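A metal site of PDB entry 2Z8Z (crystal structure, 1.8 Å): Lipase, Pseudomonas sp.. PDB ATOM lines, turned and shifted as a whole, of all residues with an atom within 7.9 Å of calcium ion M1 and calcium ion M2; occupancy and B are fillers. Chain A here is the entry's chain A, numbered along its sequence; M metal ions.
C of Gly 410 touches calcium ion M2, 3.9 Å away.
Eight residues have an atom within 4 Å of calcium ion M2: Arg 392, Ala 393, Gly 394, Asp 396, Gly 409, Gly 410, Ala 411 and Asn 414.
The nearest printed residue that does not touch calcium ion M2 is Gly 391 (4.2 Å).
The backbone carbonyl oxygen (O) of Asp 378 lies within hydrogen-bond range of the backbone NH (N) of Thr 397 (2.9 Å).
The backbone carbonyl oxygen (O) of Asp 396 lies within hydrogen-bond range of the backbone NH (N) of Thr 415, at 2.9 Å.
The side-chain hydroxyl (OG) of Ser 374 is in hydrogen-bond range of the backbone NH (N) of Ser 376 (3.0 Å).
N of Gly 391 sits at hydrogen-bond distance from O of Leu 408, 3.0 Å away.
The side-chain carboxylate (OD1) of Asp 375 lies within salt-bridge range of the guanidinium group (NE) of Arg 392, at 2.9 Å.
O of Gly 410 sits at hydrogen-bond distance from ND2 of Asn 414, at 3.1 Å.
The backbone carbonyl oxygen (O) of Gly 412 lies within hydrogen-bond range of the side-chain amide nitrogen (ND2) of Asn 414 (3.4 Å).
ND2 of Asn 414 is in hydrogen-bond range of O of Asp 449, 2.8 Å away.
Calcium ion M1 is bound by OD2 of Asp 378 (2.2 Å), O of Ala 393 (2.2 Å), O of Ser 376 (2.3 Å), O of Gly 391 (2.3 Å), O of Ser 374 (2.4 Å) and OD1 of Asp 396 (2.5 Å).
Calcium ion M1 has six donor atoms within binding distance.
Slightly farther from calcium ion M1 lies OD2 of Asp 396 (3.0 Å).
Calcium ion M2 is bound by OD2 of Asp 396 (2.3 Å), O of Ala 411 (2.3 Å), O of Gly 394 (2.3 Å), O of Arg 392 (2.3 Å), O of Gly 409 (2.4 Å) and OD1 of Asn 414 (2.5 Å).
Calcium ion M2 has six donor atoms within binding distance.
Within 4 Å of calcium ion M1: Ser 374, Ser 376, Asp 378, Gly 391, Arg 392, Ala 393 and Asp 396.
The nearest printed residue that does not touch calcium ion M1 is Asp 375 (4.1 Å).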
ATOM      1  N   ALA A 343     -18.192  -3.926  31.434  1.00  0.00           N
ATOM      2  CA  ALA A 343     -18.266  -2.798  32.310  1.00  0.00           C
ATOM      3  C   ALA A 343     -18.468  -3.286  33.751  1.00  0.00           C
ATOM      4  O   ALA A 343     -19.576  -3.757  34.128  1.00  0.00           O
ATOM      5  CB  ALA A 343     -19.420  -1.893  31.889  1.00  0.00           C
ATOM      6  N   ARG A 350     -18.564   4.805  37.838  1.00  0.00           N
ATOM      7  CA  ARG A 350     -19.366   4.685  36.620  1.00  0.00           C
ATOM      8  C   ARG A 350     -19.808   6.061  36.133  1.00  0.00           C
ATOM      9  O   ARG A 350     -19.983   6.298  34.907  1.00  0.00           O
ATOM     10  CB  ARG A 350     -20.602   3.802  36.881  1.00  0.00           C
ATOM     11  CG  ARG A 350     -21.312   3.413  35.604  1.00  0.00           C
ATOM     12  CD  ARG A 350     -22.441   2.464  35.879  1.00  0.00           C
ATOM     13  NE  ARG A 350     -23.301   2.979  36.935  1.00  0.00           N
ATOM     14  CZ  ARG A 350     -23.568   2.383  38.088  1.00  0.00           C
ATOM     15  NH1 ARG A 350     -23.086   1.184  38.384  1.00  0.00           N
ATOM     16  NH2 ARG A 350     -24.376   2.999  38.938  1.00  0.00           N
ATOM     17  N   ILE A 372     -19.556  -4.392  26.638  1.00  0.00           N
ATOM     18  CA  ILE A 372     -20.844  -4.724  27.239  1.00  0.00           C
ATOM     19  C   ILE A 372     -21.092  -3.856  28.475  1.00  0.00           C
ATOM     20  O   ILE A 372     -20.368  -3.939  29.471  1.00  0.00           O
ATOM     21  CB  ILE A 372     -20.909  -6.210  27.683  1.00  0.00           C
ATOM     22  CG1 ILE A 372     -20.477  -7.148  26.547  1.00  0.00           C
ATOM     23  CG2 ILE A 372     -22.322  -6.614  28.077  1.00  0.00           C
ATOM     24  CD1 ILE A 372     -21.166  -6.882  25.297  1.00  0.00           C
ATOM     25  N   GLY A 373     -22.177  -3.117  28.447  1.00  0.00           N
ATOM     26  CA  GLY A 373     -22.524  -2.237  29.577  1.00  0.00           C
ATOM     27  C   GLY A 373     -23.156  -2.910  30.778  1.00  0.00           C
ATOM     28  O   GLY A 373     -23.293  -4.130  30.814  1.00  0.00           O
ATOM     29  N   SER A 374     -23.550  -2.099  31.784  1.00  0.00           N
ATOM     30  CA  SER A 374     -24.273  -2.542  32.971  1.00  0.00           C
ATOM     31  C   SER A 374     -25.712  -2.158  32.828  1.00  0.00           C
ATOM     32  O   SER A 374     -26.079  -1.430  31.909  1.00  0.00           O
ATOM     33  CB  SER A 374     -23.750  -1.865  34.231  1.00  0.00           C
ATOM     34  OG  SER A 374     -24.085  -0.496  34.292  1.00  0.00           O
ATOM     35  N   ASP A 375     -26.525  -2.582  33.772  1.00  0.00           N
ATOM     36  CA  ASP A 375     -27.896  -2.154  33.787  1.00  0.00           C
ATOM     37  C   ASP A 375     -28.137  -0.741  34.303  1.00  0.00           C
ATOM     38  O   ASP A 375     -29.303  -0.307  34.356  1.00  0.00           O
ATOM     39  CB  ASP A 375     -28.713  -3.191  34.505  1.00  0.00           C
ATOM     40  CG  ASP A 375     -28.981  -4.405  33.603  1.00  0.00           C
ATOM     41  OD1 ASP A 375     -29.070  -4.286  32.344  1.00  0.00           O
ATOM     42  OD2 ASP A 375     -29.144  -5.420  34.173  1.00  0.00           O
ATOM     43  N   SER A 376     -27.069  -0.028  34.607  1.00  0.00           N
ATOM     44  CA  SER A 376     -27.190   1.380  35.008  1.00  0.00           C
ATOM     45  C   SER A 376     -26.678   2.311  33.903  1.00  0.00           C
ATOM     46  O   SER A 376     -26.392   1.885  32.754  1.00  0.00           O
ATOM     47  CB  SER A 376     -26.426   1.571  36.296  1.00  0.00           C
ATOM     48  OG  SER A 376     -26.916   0.670  37.277  1.00  0.00           O
ATOM     49  N   ASN A 377     -26.605   3.609  34.206  1.00  0.00           N
ATOM     50  CA  ASN A 377     -26.147   4.589  33.241  1.00  0.00           C
ATOM     51  C   ASN A 377     -24.656   4.479  33.002  1.00  0.00           C
ATOM     52  O   ASN A 377     -23.877   4.727  33.934  1.00  0.00           O
ATOM     53  CB  ASN A 377     -26.414   6.004  33.801  1.00  0.00           C
ATOM     54  CG  ASN A 377     -27.865   6.266  33.998  1.00  0.00           C
ATOM     55  OD1 ASN A 377     -28.670   5.427  33.717  1.00  0.00           O
ATOM     56  ND2 ASN A 377     -28.198   7.471  34.481  1.00  0.00           N
ATOM     57  N   ASP A 378     -24.271   4.110  31.777  1.00  0.00           N
ATOM     58  CA  ASP A 378     -22.870   3.919  31.392  1.00  0.00           C
ATOM     59  C   ASP A 378     -22.391   5.005  30.441  1.00  0.00           C
ATOM     60  O   ASP A 378     -23.205   5.536  29.689  1.00  0.00           O
ATOM     61  CB  ASP A 378     -22.765   2.554  30.652  1.00  0.00           C
ATOM     62  CG  ASP A 378     -23.249   1.394  31.508  1.00  0.00           C
ATOM     63  OD1 ASP A 378     -22.673   1.235  32.621  1.00  0.00           O
ATOM     64  OD2 ASP A 378     -24.199   0.643  31.087  1.00  0.00           O
ATOM     65  N   LEU A 379     -21.068   5.255  30.445  1.00  0.00           N
ATOM     66  CA  LEU A 379     -20.295   6.039  29.482  1.00  0.00           C
ATOM     67  C   LEU A 379     -19.431   4.986  28.802  1.00  0.00           C
ATOM     68  O   LEU A 379     -18.607   4.345  29.445  1.00  0.00           O
ATOM     69  CB  LEU A 379     -19.375   7.110  30.151  1.00  0.00           C
ATOM     70  CG  LEU A 379     -20.145   8.055  31.094  1.00  0.00           C
ATOM     71  CD1 LEU A 379     -19.193   8.958  31.841  1.00  0.00           C
ATOM     72  CD2 LEU A 379     -21.139   8.859  30.307  1.00  0.00           C
ATOM     73  N   ILE A 380     -19.733   4.755  27.526  1.00  0.00           N
ATOM     74  CA  ILE A 380     -19.068   3.738  26.725  1.00  0.00           C
ATOM     75  C   ILE A 380     -18.309   4.363  25.532  1.00  0.00           C
ATOM     76  O   ILE A 380     -18.890   5.086  24.699  1.00  0.00           O
ATOM     77  CB  ILE A 380     -20.100   2.676  26.273  1.00  0.00           C
ATOM     78  CG1 ILE A 380     -20.660   1.890  27.492  1.00  0.00           C
ATOM     79  CG2 ILE A 380     -19.483   1.750  25.280  1.00  0.00           C
ATOM     80  CD1 ILE A 380     -21.816   1.058  27.226  1.00  0.00           C
ATOM     81  N   GLU A 390     -22.839  -2.134  23.612  1.00  0.00           N
ATOM     82  CA  GLU A 390     -24.152  -2.539  24.119  1.00  0.00           C
ATOM     83  C   GLU A 390     -24.377  -1.868  25.482  1.00  0.00           C
ATOM     84  O   GLU A 390     -23.651  -2.124  26.447  1.00  0.00           O
ATOM     85  CB  GLU A 390     -24.238  -4.068  24.255  1.00  0.00           C
ATOM     86  CG  GLU A 390     -25.631  -4.523  24.700  1.00  0.00           C
ATOM     87  CD  GLU A 390     -25.778  -6.032  24.693  1.00  0.00           C
ATOM     88  OE1 GLU A 390     -24.777  -6.694  25.177  1.00  0.00           O
ATOM     89  OE2 GLU A 390     -26.858  -6.529  24.257  1.00  0.00           O
ATOM     90  N   GLY A 391     -25.382  -0.993  25.527  1.00  0.00           N
ATOM     91  CA  GLY A 391     -25.724  -0.224  26.714  1.00  0.00           C
ATOM     92  C   GLY A 391     -26.515  -0.960  27.781  1.00  0.00           C
ATOM     93  O   GLY A 391     -26.287  -0.695  28.965  1.00  0.00           O
ATOM     94  N   ARG A 392     -27.360  -1.900  27.373  1.00  0.00           N
ATOM     95  CA  ARG A 392     -28.347  -2.498  28.232  1.00  0.00           C
ATOM     96  C   ARG A 392     -29.197  -1.386  28.906  1.00  0.00           C
ATOM     97  O   ARG A 392     -29.301  -0.320  28.343  1.00  0.00           O
ATOM     98  CB  ARG A 392     -27.689  -3.455  29.268  1.00  0.00           C
ATOM     99  CG  ARG A 392     -26.780  -4.541  28.674  1.00  0.00           C
ATOM    100  CD  ARG A 392     -26.138  -5.440  29.811  1.00  0.00           C
ATOM    101  NE  ARG A 392     -27.158  -5.851  30.795  1.00  0.00           N
ATOM    102  CZ  ARG A 392     -27.769  -7.038  30.792  1.00  0.00           C
ATOM    103  NH1 ARG A 392     -27.465  -7.934  29.877  1.00  0.00           N
ATOM    104  NH2 ARG A 392     -28.615  -7.378  31.730  1.00  0.00           N
ATOM    105  N   ALA A 393     -29.817  -1.658  30.062  1.00  0.00           N
ATOM    106  CA  ALA A 393     -30.672  -0.672  30.684  1.00  0.00           C
ATOM    107  C   ALA A 393     -29.869   0.488  31.178  1.00  0.00           C
ATOM    108  O   ALA A 393     -28.570   0.515  31.145  1.00  0.00           O
ATOM    109  CB  ALA A 393     -31.478  -1.309  31.812  1.00  0.00           C
ATOM    110  N   GLY A 394     -30.595   1.507  31.634  1.00  0.00           N
ATOM    111  CA  GLY A 394     -29.936   2.710  32.052  1.00  0.00           C
ATOM    112  C   GLY A 394     -29.795   3.644  30.852  1.00  0.00           C
ATOM    113  O   GLY A 394     -29.982   3.246  29.686  1.00  0.00           O
ATOM    114  N   ASN A 395     -29.554   4.909  31.155  1.00  0.00           N
ATOM    115  CA  ASN A 395     -29.422   5.977  30.163  1.00  0.00           C
ATOM    116  C   ASN A 395     -27.938   5.973  29.848  1.00  0.00           C
ATOM    117  O   ASN A 395     -27.124   6.413  30.648  1.00  0.00           O
ATOM    118  CB  ASN A 395     -29.785   7.313  30.752  1.00  0.00           C
ATOM    119  CG  ASN A 395     -31.280   7.430  31.061  1.00  0.00           C
ATOM    120  OD1 ASN A 395     -32.076   6.598  30.643  1.00  0.00           O
ATOM    121  ND2 ASN A 395     -31.644   8.461  31.836  1.00  0.00           N
ATOM    122  N   ASP A 396     -27.592   5.481  28.657  1.00  0.00           N
ATOM    123  CA  ASP A 396     -26.170   5.276  28.304  1.00  0.00           C
ATOM    124  C   ASP A 396     -25.739   6.312  27.307  1.00  0.00           C
ATOM    125  O   ASP A 396     -26.519   6.666  26.429  1.00  0.00           O
ATOM    126  CB  ASP A 396     -25.998   3.855  27.694  1.00  0.00           C
ATOM    127  CG  ASP A 396     -26.464   2.800  28.647  1.00  0.00           C
ATOM    128  OD1 ASP A 396     -25.938   2.846  29.778  1.00  0.00           O
ATOM    129  OD2 ASP A 396     -27.415   2.037  28.342  1.00  0.00           O
ATOM    130  N   THR A 397     -24.463   6.734  27.410  1.00  0.00           N
ATOM    131  CA  THR A 397     -23.887   7.652  26.477  1.00  0.00           C
ATOM    132  C   THR A 397     -22.709   6.981  25.756  1.00  0.00           C
ATOM    133  O   THR A 397     -21.868   6.386  26.427  1.00  0.00           O
ATOM    134  CB  THR A 397     -23.400   8.923  27.166  1.00  0.00           C
ATOM    135  OG1 THR A 397     -24.526   9.512  27.860  1.00  0.00           O
ATOM    136  CG2 THR A 397     -22.920   9.867  26.145  1.00  0.00           C
ATOM    137  N   PHE A 398     -22.729   7.036  24.422  1.00  0.00           N
ATOM    138  CA  PHE A 398     -21.688   6.402  23.602  1.00  0.00           C
ATOM    139  C   PHE A 398     -20.857   7.408  22.849  1.00  0.00           C
ATOM    140  O   PHE A 398     -21.357   8.398  22.326  1.00  0.00           O
ATOM    141  CB  PHE A 398     -22.296   5.440  22.585  1.00  0.00           C
ATOM    142  CG  PHE A 398     -23.187   4.386  23.170  1.00  0.00           C
ATOM    143  CD1 PHE A 398     -22.707   3.134  23.499  1.00  0.00           C
ATOM    144  CD2 PHE A 398     -24.538   4.642  23.369  1.00  0.00           C
ATOM    145  CE1 PHE A 398     -23.617   2.140  24.031  1.00  0.00           C
ATOM    146  CE2 PHE A 398     -25.386   3.689  23.874  1.00  0.00           C
ATOM    147  CZ  PHE A 398     -24.908   2.407  24.210  1.00  0.00           C
ATOM    148  N   LEU A 408     -26.049  -0.466  20.305  1.00  0.00           N
ATOM    149  CA  LEU A 408     -27.379  -0.823  20.792  1.00  0.00           C
ATOM    150  C   LEU A 408     -27.620  -0.051  22.102  1.00  0.00           C
ATOM    151  O   LEU A 408     -27.086  -0.370  23.133  1.00  0.00           O
ATOM    152  CB  LEU A 408     -27.522  -2.301  21.036  1.00  0.00           C
ATOM    153  CG  LEU A 408     -27.238  -3.214  19.796  1.00  0.00           C
ATOM    154  CD1 LEU A 408     -27.291  -4.703  20.147  1.00  0.00           C
ATOM    155  CD2 LEU A 408     -28.285  -2.872  18.753  1.00  0.00           C
ATOM    156  N   GLY A 409     -28.452   0.960  22.033  1.00  0.00           N
ATOM    157  CA  GLY A 409     -28.767   1.671  23.242  1.00  0.00           C
ATOM    158  C   GLY A 409     -29.427   0.884  24.348  1.00  0.00           C
ATOM    159  O   GLY A 409     -29.263   1.252  25.514  1.00  0.00           O
ATOM    160  N   GLY A 410     -30.223  -0.126  24.003  1.00  0.00           N
ATOM    161  CA  GLY A 410     -31.092  -0.835  24.949  1.00  0.00           C
ATOM    162  C   GLY A 410     -32.192   0.027  25.544  1.00  0.00           C
ATOM    163  O   GLY A 410     -32.559   1.080  24.981  1.00  0.00           O
ATOM    164  N   ALA A 411     -32.739  -0.413  26.669  1.00  0.00           N
ATOM    165  CA  ALA A 411     -33.669   0.370  27.451  1.00  0.00           C
ATOM    166  C   ALA A 411     -33.093   1.688  27.850  1.00  0.00           C
ATOM    167  O   ALA A 411     -31.897   1.923  27.799  1.00  0.00           O
ATOM    168  CB  ALA A 411     -34.126  -0.401  28.677  1.00  0.00           C
ATOM    169  N   GLY A 412     -33.954   2.614  28.229  1.00  0.00           N
ATOM    170  CA  GLY A 412     -33.495   3.937  28.660  1.00  0.00           C
ATOM    171  C   GLY A 412     -33.489   5.036  27.591  1.00  0.00           C
ATOM    172  O   GLY A 412     -33.851   4.817  26.431  1.00  0.00           O
ATOM    173  N   ASN A 413     -33.053   6.216  28.017  1.00  0.00           N
ATOM    174  CA  ASN A 413     -32.848   7.352  27.114  1.00  0.00           C
ATOM    175  C   ASN A 413     -31.371   7.443  26.850  1.00  0.00           C
ATOM    176  O   ASN A 413     -30.591   7.874  27.728  1.00  0.00           O
ATOM    177  CB  ASN A 413     -33.341   8.656  27.746  1.00  0.00           C
ATOM    178  CG  ASN A 413     -34.800   8.621  28.036  1.00  0.00           C
ATOM    179  OD1 ASN A 413     -35.618   8.140  27.236  1.00  0.00           O
ATOM    180  ND2 ASN A 413     -35.158   9.095  29.233  1.00  0.00           N
ATOM    181  N   ASN A 414     -30.988   7.038  25.644  1.00  0.00           N
ATOM    182  CA  ASN A 414     -29.600   6.897  25.290  1.00  0.00           C
ATOM    183  C   ASN A 414     -29.135   7.966  24.313  1.00  0.00           C
ATOM    184  O   ASN A 414     -29.928   8.433  23.512  1.00  0.00           O
ATOM    185  CB  ASN A 414     -29.348   5.478  24.671  1.00  0.00           C
ATOM    186  CG  ASN A 414     -29.970   4.382  25.496  1.00  0.00           C
ATOM    187  OD1 ASN A 414     -29.542   4.142  26.613  1.00  0.00           O
ATOM    188  ND2 ASN A 414     -30.996   3.707  24.940  1.00  0.00           N
ATOM    189  N   THR A 415     -27.839   8.241  24.325  1.00  0.00           N
ATOM    190  CA  THR A 415     -27.197   9.279  23.563  1.00  0.00           C
ATOM    191  C   THR A 415     -25.920   8.818  22.843  1.00  0.00           C
ATOM    192  O   THR A 415     -25.102   8.082  23.395  1.00  0.00           O
ATOM    193  CB  THR A 415     -26.797  10.416  24.562  1.00  0.00           C
ATOM    194  OG1 THR A 415     -28.000  10.856  25.217  1.00  0.00           O
ATOM    195  CG2 THR A 415     -26.155  11.612  23.856  1.00  0.00           C
ATOM    196  N   ASP A 449     -32.225   2.367  19.356  1.00  0.00           N
ATOM    197  CA  ASP A 449     -32.637   2.914  20.666  1.00  0.00           C
ATOM    198  C   ASP A 449     -31.769   4.076  21.101  1.00  0.00           C
ATOM    199  O   ASP A 449     -31.542   4.251  22.255  1.00  0.00           O
ATOM    200  CB  ASP A 449     -32.651   1.764  21.696  1.00  0.00           C
ATOM    201  CG  ASP A 449     -33.630   0.673  21.307  1.00  0.00           C
ATOM    202  OD1 ASP A 449     -34.816   0.998  21.120  1.00  0.00           O
ATOM    203  OD2 ASP A 449     -33.254  -0.485  21.150  1.00  0.00           O
ATOM    204  N   ILE A 450     -31.362   4.909  20.156  1.00  0.00           N
ATOM    205  CA  ILE A 450     -30.631   6.116  20.481  1.00  0.00           C
ATOM    206  C   ILE A 450     -31.554   7.306  20.111  1.00  0.00           C
ATOM    207  O   ILE A 450     -31.899   7.507  18.943  1.00  0.00           O
ATOM    208  CB  ILE A 450     -29.203   6.106  19.875  1.00  0.00           C
ATOM    209  CG1 ILE A 450     -28.346   5.197  20.826  1.00  0.00           C
ATOM    210  CG2 ILE A 450     -28.715   7.594  19.767  1.00  0.00           C
ATOM    211  CD1 ILE A 450     -27.054   4.726  20.406  1.00  0.00           C
HETATM  212 CA    CA M   1     -26.376   0.668  30.831  1.00  0.00          CA
HETATM  213 CA    CA M   2     -29.618   1.941  27.797  1.00  0.00          CA
